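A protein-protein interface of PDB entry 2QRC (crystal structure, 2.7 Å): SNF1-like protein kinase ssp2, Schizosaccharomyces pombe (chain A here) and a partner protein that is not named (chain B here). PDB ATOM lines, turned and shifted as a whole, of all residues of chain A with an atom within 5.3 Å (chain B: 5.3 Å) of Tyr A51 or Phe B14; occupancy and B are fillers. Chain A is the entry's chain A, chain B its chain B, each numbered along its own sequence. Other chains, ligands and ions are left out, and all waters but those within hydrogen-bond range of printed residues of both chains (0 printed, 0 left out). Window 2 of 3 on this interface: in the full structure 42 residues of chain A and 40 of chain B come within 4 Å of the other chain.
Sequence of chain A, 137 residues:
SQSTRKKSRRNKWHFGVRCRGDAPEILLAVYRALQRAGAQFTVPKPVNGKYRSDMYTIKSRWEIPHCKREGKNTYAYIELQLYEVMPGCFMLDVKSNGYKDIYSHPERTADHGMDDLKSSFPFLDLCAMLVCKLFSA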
ATOM      1  N   PRO A  44      -2.804 -30.115  22.245  1.00  0.00           N
ATOM      2  CA  PRO A  44      -1.360 -29.959  22.465  1.00  0.00           C
ATOM      3  C   PRO A  44      -0.971 -29.893  23.934  1.00  0.00           C
ATOM      4  O   PRO A  44      -1.755 -29.439  24.774  1.00  0.00           O
ATOM      5  CB  PRO A  44      -1.032 -28.618  21.796  1.00  0.00           C
ATOM      6  CG  PRO A  44      -2.196 -28.308  20.921  1.00  0.00           C
ATOM      7  CD  PRO A  44      -3.387 -28.947  21.558  1.00  0.00           C
ATOM      8  N   LYS A  45       0.245 -30.356  24.213  1.00  0.00           N
ATOM      9  CA  LYS A  45       0.872 -30.221  25.518  1.00  0.00           C
ATOM     10  C   LYS A  45       2.343 -29.769  25.349  1.00  0.00           C
ATOM     11  O   LYS A  45       3.157 -30.520  24.806  1.00  0.00           O
ATOM     12  CB  LYS A  45       0.761 -31.539  26.309  1.00  0.00           C
ATOM     13  CG  LYS A  45       1.767 -31.691  27.482  1.00  0.00           C
ATOM     14  CD  LYS A  45       1.775 -30.481  28.430  1.00  0.00           C
ATOM     15  CE  LYS A  45       0.634 -30.510  29.448  1.00  0.00           C
ATOM     16  NZ  LYS A  45       1.123 -31.102  30.788  1.00  0.00           N
ATOM     17  N   PRO A  46       2.688 -28.551  25.826  1.00  0.00           N
ATOM     18  CA  PRO A  46       4.006 -27.980  25.562  1.00  0.00           C
ATOM     19  C   PRO A  46       5.157 -28.653  26.339  1.00  0.00           C
ATOM     20  O   PRO A  46       4.905 -29.356  27.323  1.00  0.00           O
ATOM     21  CB  PRO A  46       3.832 -26.522  25.993  1.00  0.00           C
ATOM     22  CG  PRO A  46       2.791 -26.545  27.018  1.00  0.00           C
ATOM     23  CD  PRO A  46       1.855 -27.643  26.639  1.00  0.00           C
ATOM     24  N   VAL A  47       6.401 -28.435  25.888  1.00  0.00           N
ATOM     25  CA  VAL A  47       7.612 -28.947  26.567  1.00  0.00           C
ATOM     26  C   VAL A  47       8.177 -27.964  27.624  1.00  0.00           C
ATOM     27  O   VAL A  47       9.178 -27.259  27.388  1.00  0.00           O
ATOM     28  CB  VAL A  47       8.729 -29.407  25.557  1.00  0.00           C
ATOM     29  CG1 VAL A  47       9.125 -28.279  24.536  1.00  0.00           C
ATOM     30  CG2 VAL A  47       9.983 -30.030  26.363  1.00  0.00           C
ATOM     31  N   GLY A  49       7.778 -25.084  28.224  1.00  0.00           N
ATOM     32  CA  GLY A  49       7.344 -23.819  27.619  1.00  0.00           C
ATOM     33  C   GLY A  49       5.905 -23.809  27.120  1.00  0.00           C
ATOM     34  O   GLY A  49       4.998 -23.674  27.939  1.00  0.00           O
ATOM     35  N   LYS A  50       5.631 -23.949  25.815  1.00  0.00           N
ATOM     36  CA  LYS A  50       6.528 -24.208  24.652  1.00  0.00           C
ATOM     37  C   LYS A  50       5.933 -25.295  23.734  1.00  0.00           C
ATOM     38  O   LYS A  50       6.097 -26.500  23.965  1.00  0.00           O
ATOM     39  CB  LYS A  50       7.986 -24.517  25.005  1.00  0.00           C
ATOM     40  CG  LYS A  50       8.954 -23.430  24.532  1.00  0.00           C
ATOM     41  CD  LYS A  50      10.203 -23.321  25.424  1.00  0.00           C
ATOM     42  CE  LYS A  50      11.038 -22.107  25.050  1.00  0.00           C
ATOM     43  NZ  LYS A  50      12.362 -22.124  25.718  1.00  0.00           N
ATOM     44  N   TYR A  51       5.238 -24.866  22.688  1.00  0.00           N
ATOM     45  CA  TYR A  51       4.464 -25.811  21.885  1.00  0.00           C
ATOM     46  C   TYR A  51       5.258 -26.620  20.854  1.00  0.00           C
ATOM     47  O   TYR A  51       6.067 -26.081  20.088  1.00  0.00           O
ATOM     48  CB  TYR A  51       3.200 -25.157  21.306  1.00  0.00           C
ATOM     49  CG  TYR A  51       2.124 -25.007  22.356  1.00  0.00           C
ATOM     50  CD1 TYR A  51       1.924 -23.784  23.016  1.00  0.00           C
ATOM     51  CD2 TYR A  51       1.338 -26.102  22.729  1.00  0.00           C
ATOM     52  CE1 TYR A  51       0.945 -23.651  24.002  1.00  0.00           C
ATOM     53  CE2 TYR A  51       0.361 -25.981  23.715  1.00  0.00           C
ATOM     54  CZ  TYR A  51       0.170 -24.758  24.346  1.00  0.00           C
ATOM     55  OH  TYR A  51      -0.798 -24.651  25.317  1.00  0.00           O
ATOM     56  N   ARG A  52       5.012 -27.928  20.880  1.00  0.00           N
ATOM     57  CA  ARG A  52       5.716 -28.909  20.064  1.00  0.00           C
ATOM     58  C   ARG A  52       4.995 -29.157  18.744  1.00  0.00           C
ATOM     59  O   ARG A  52       3.769 -29.338  18.701  1.00  0.00           O
ATOM     60  CB  ARG A  52       5.912 -30.231  20.838  1.00  0.00           C
ATOM     61  CG  ARG A  52       4.636 -30.851  21.507  1.00  0.00           C
ATOM     62  CD  ARG A  52       4.980 -32.118  22.342  1.00  0.00           C
ATOM     63  NE  ARG A  52       3.970 -32.431  23.362  1.00  0.00           N
ATOM     64  CZ  ARG A  52       3.045 -33.390  23.273  1.00  0.00           C
ATOM     65  NH1 ARG A  52       2.968 -34.180  22.206  1.00  0.00           N
ATOM     66  NH2 ARG A  52       2.187 -33.563  24.271  1.00  0.00           N
ATOM     67  N   SER A  53       5.781 -29.170  17.672  1.00  0.00           N
ATOM     68  CA  SER A  53       5.284 -29.319  16.310  1.00  0.00           C
ATOM     69  C   SER A  53       4.218 -30.399  16.103  1.00  0.00           C
ATOM     70  O   SER A  53       3.493 -30.370  15.115  1.00  0.00           O
ATOM     71  CB  SER A  53       6.465 -29.587  15.391  1.00  0.00           C
ATOM     72  OG  SER A  53       6.048 -30.379  14.310  1.00  0.00           O
ATOM     73  N   MET A  55       1.629 -30.747  17.612  1.00  0.00           N
ATOM     74  CA  MET A  55       0.310 -30.196  17.870  1.00  0.00           C
ATOM     75  C   MET A  55      -0.603 -30.322  16.642  1.00  0.00           C
ATOM     76  O   MET A  55      -1.815 -30.384  16.785  1.00  0.00           O
ATOM     77  CB  MET A  55       0.388 -28.757  18.426  1.00  0.00           C
ATOM     78  CG  MET A  55       0.562 -27.616  17.431  1.00  0.00           C
ATOM     79  SD  MET A  55       0.644 -26.009  18.299  1.00  0.00           S
ATOM     80  CE  MET A  55       1.175 -24.942  16.954  1.00  0.00           C
ATOM     81  N   PRO B  12      -8.730 -25.820  22.653  1.00  0.00           N
ATOM     82  CA  PRO B  12      -7.609 -25.353  23.485  1.00  0.00           C
ATOM     83  C   PRO B  12      -7.634 -23.838  23.586  1.00  0.00           C
ATOM     84  O   PRO B  12      -7.837 -23.152  22.573  1.00  0.00           O
ATOM     85  CB  PRO B  12      -6.366 -25.824  22.730  1.00  0.00           C
ATOM     86  CG  PRO B  12      -6.832 -26.959  21.905  1.00  0.00           C
ATOM     87  CD  PRO B  12      -8.267 -26.641  21.518  1.00  0.00           C
ATOM     88  N   ALA B  13      -7.456 -23.335  24.807  1.00  0.00           N
ATOM     89  CA  ALA B  13      -7.659 -21.922  25.097  1.00  0.00           C
ATOM     90  C   ALA B  13      -6.719 -20.997  24.324  1.00  0.00           C
ATOM     91  O   ALA B  13      -7.161 -19.981  23.787  1.00  0.00           O
ATOM     92  CB  ALA B  13      -7.565 -21.666  26.593  1.00  0.00           C
ATOM     93  N   PHE B  14      -5.442 -21.365  24.241  1.00  0.00           N
ATOM     94  CA  PHE B  14      -4.416 -20.490  23.679  1.00  0.00           C
ATOM     95  C   PHE B  14      -4.690 -20.101  22.234  1.00  0.00           C
ATOM     96  O   PHE B  14      -4.231 -19.055  21.767  1.00  0.00           O
ATOM     97  CB  PHE B  14      -3.022 -21.107  23.823  1.00  0.00           C
ATOM     98  CG  PHE B  14      -2.772 -22.259  22.904  1.00  0.00           C
ATOM     99  CD1 PHE B  14      -3.086 -23.557  23.296  1.00  0.00           C
ATOM    100  CD2 PHE B  14      -2.223 -22.051  21.642  1.00  0.00           C
ATOM    101  CE1 PHE B  14      -2.865 -24.633  22.442  1.00  0.00           C
ATOM    102  CE2 PHE B  14      -1.994 -23.119  20.777  1.00  0.00           C
ATOM    103  CZ  PHE B  14      -2.317 -24.415  21.177  1.00  0.00           C
ATOM    104  N   LEU B  15      -5.438 -20.950  21.534  1.00  0.00           N
ATOM    105  CA  LEU B  15      -5.947 -20.631  20.205  1.00  0.00           C
ATOM    106  C   LEU B  15      -7.174 -19.713  20.304  1.00  0.00           C
ATOM    107  O   LEU B  15      -8.178 -19.927  19.625  1.00  0.00           O
ATOM    108  CB  LEU B  15      -6.288 -21.913  19.441  1.00  0.00           C
ATOM    109  CG  LEU B  15      -5.210 -23.001  19.338  1.00  0.00           C
ATOM    110  CD1 LEU B  15      -5.808 -24.398  19.325  1.00  0.00           C
ATOM    111  CD2 LEU B  15      -4.327 -22.795  18.124  1.00  0.00           C
ATOM    112  N   THR B  16      -7.086 -18.712  21.187  1.00  0.00           N
ATOM    113  CA  THR B  16      -8.030 -17.590  21.252  1.00  0.00           C
ATOM    114  C   THR B  16      -7.396 -16.367  21.942  1.00  0.00           C
ATOM    115  O   THR B  16      -8.075 -15.366  22.181  1.00  0.00           O
ATOM    116  CB  THR B  16      -9.409 -17.995  21.842  1.00  0.00           C
ATOM    117  OG1 THR B  16      -9.612 -19.407  21.725  1.00  0.00           O
ATOM    118  CG2 THR B  16     -10.528 -17.255  21.121  1.00  0.00           C
ATOM    119  N   SER B  17      -6.092 -16.423  22.204  1.00  0.00           N
ATOM    120  CA  SER B  17      -5.409 -15.427  23.044  1.00  0.00           C
ATOM    121  C   SER B  17      -5.795 -13.955  22.810  1.00  0.00           C
ATOM    122  O   SER B  17      -6.513 -13.361  23.612  1.00  0.00           O
ATOM    123  CB  SER B  17      -3.893 -15.595  22.950  1.00  0.00           C
ATOM    124  OG  SER B  17      -3.407 -16.431  23.986  1.00  0.00           O
ATOM    125  N   THR B  19      -4.259 -13.645  18.296  1.00  0.00           N
ATOM    126  CA  THR B  19      -3.644 -14.973  18.266  1.00  0.00           C
ATOM    127  C   THR B  19      -2.422 -14.807  17.362  1.00  0.00           C
ATOM    128  O   THR B  19      -1.654 -15.742  17.139  1.00  0.00           O
ATOM    129  CB  THR B  19      -4.551 -16.070  17.630  1.00  0.00           C
ATOM    130  OG1 THR B  19      -5.938 -15.744  17.795  1.00  0.00           O
ATOM    131  CG2 THR B  19      -4.260 -17.456  18.239  1.00  0.00           C
ATOM    132  N   GLU B  22       2.690 -14.142  18.492  1.00  0.00           N
ATOM    133  CA  GLU B  22       2.066 -14.958  19.526  1.00  0.00           C
ATOM    134  C   GLU B  22       2.717 -16.335  19.611  1.00  0.00           C
ATOM    135  O   GLU B  22       2.500 -17.187  18.750  1.00  0.00           O
ATOM    136  CB  GLU B  22       0.566 -15.100  19.265  1.00  0.00           C
ATOM    137  CG  GLU B  22      -0.064 -16.321  19.913  1.00  0.00           C
ATOM    138  CD  GLU B  22      -0.382 -16.105  21.380  1.00  0.00           C
ATOM    139  OE1 GLU B  22      -0.176 -14.975  21.873  1.00  0.00           O
ATOM    140  OE2 GLU B  22      -0.837 -17.062  22.039  1.00  0.00           O
ATOM    141  N   LEU B  23       3.515 -16.545  20.652  1.00  0.00           N
ATOM    142  CA  LEU B  23       4.305 -17.763  20.780  1.00  0.00           C
ATOM    143  C   LEU B  23       5.271 -17.699  19.601  1.00  0.00           C
ATOM    144  O   LEU B  23       6.484 -17.812  19.773  1.00  0.00           O
ATOM    145  CB  LEU B  23       3.511 -18.842  21.517  1.00  0.00           C
ATOM    146  CG  LEU B  23       4.074 -19.297  22.865  1.00  0.00           C
ATOM    147  CD1 LEU B  23       4.397 -18.098  23.744  1.00  0.00           C
ATOM    148  CD2 LEU B  23       3.103 -20.234  23.565  1.00  0.00           C
ATOM    149  N   LEU B  25       4.579 -19.895  17.108  1.00  0.00           N
ATOM    150  CA  LEU B  25       4.553 -21.340  17.288  1.00  0.00           C
ATOM    151  C   LEU B  25       5.189 -22.100  16.146  1.00  0.00           C
ATOM    152  O   LEU B  25       5.496 -21.514  15.103  1.00  0.00           O
ATOM    153  CB  LEU B  25       3.118 -21.816  17.505  1.00  0.00           C
ATOM    154  CG  LEU B  25       2.327 -21.136  18.614  1.00  0.00           C
ATOM    155  CD1 LEU B  25       1.402 -20.108  18.011  1.00  0.00           C
ATOM    156  CD2 LEU B  25       1.530 -22.149  19.385  1.00  0.00           C
ATOM    157  N   PRO B  26       5.381 -23.419  16.335  1.00  0.00           N
ATOM    158  CA  PRO B  26       6.071 -24.255  15.361  1.00  0.00           C
ATOM    159  C   PRO B  26       5.254 -24.419  14.091  1.00  0.00           C
ATOM    160  O   PRO B  26       4.029 -24.247  14.113  1.00  0.00           O
ATOM    161  CB  PRO B  26       6.173 -25.596  16.082  1.00  0.00           C
ATOM    162  CG  PRO B  26       4.972 -25.610  16.979  1.00  0.00           C
ATOM    163  CD  PRO B  26       4.921 -24.210  17.491  1.00  0.00           C
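The guanidinium group (NE) of Arg A52 lies within hydrogen-bond range of the backbone carbonyl oxygen (O) of Lys A45, at 2.5 Å.
Pro B12 touches Pro A44. Pro A44 touches Phe B14. OH of Tyr A51 touches CD1 of Phe B14 (3.2 Å). CD1 of Tyr A51 touches CD2 of Leu B23 (3.8 Å). CB of Tyr A51 touches CD2 of Leu B25, 3.9 Å away. Pro B26 touches Tyr A51. C of Arg A52 touches CG of Pro B26 (3.96 Å). N of Ser A53 touches CG of Pro B26 (3.7 Å). CE of Met A55 touches CD2 of Leu B25, at 3.7 Å. Met A55 touches Pro B26.
Of chain B, only Phe B14 (3.2 Å), Leu B23 (3.8 Å), Leu B25 (3.9 Å) and Pro B26 (3.3 Å) come within 4 Å of Tyr A51. Printed residues of chain A within 4 Å of Pro B12: Pro A44 (3.99 Å). Of the printed residues of chain A, Leu B23 touches Tyr A51. The nearest printed residue of chain B that does not touch Tyr A51 is Pro B12 (6.3 Å). The nearest residue of chain A that does not touch Phe B14 is Met A55 (4.4 Å). The nearest printed residue of chain A that does not touch Leu B25 is Arg A52 (6.9 Å).
Of the 10 printed residues of chain A, 5 touch a printed residue of chain B. Hydrophobic or aromatic side chains of chain A that line the printed part of chain B: Pro A44, Tyr A51 and Met A55. Printed residues of chain B that touch a printed residue of chain A: Pro B12, Phe B14, Leu B23, Leu B25 and Pro B26. Hydrophobic or aromatic side chains of chain B within 4 Å of the printed part of chain A: Pro B12, Phe B14, Leu B23, Leu B25 and Pro B26. Among the printed residues, 10 pairs touch across the chains. Among the printed residues, no Asp or Glu carboxylate lies within 4 Å of a Lys or Arg side-chain nitrogen of the other chain.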
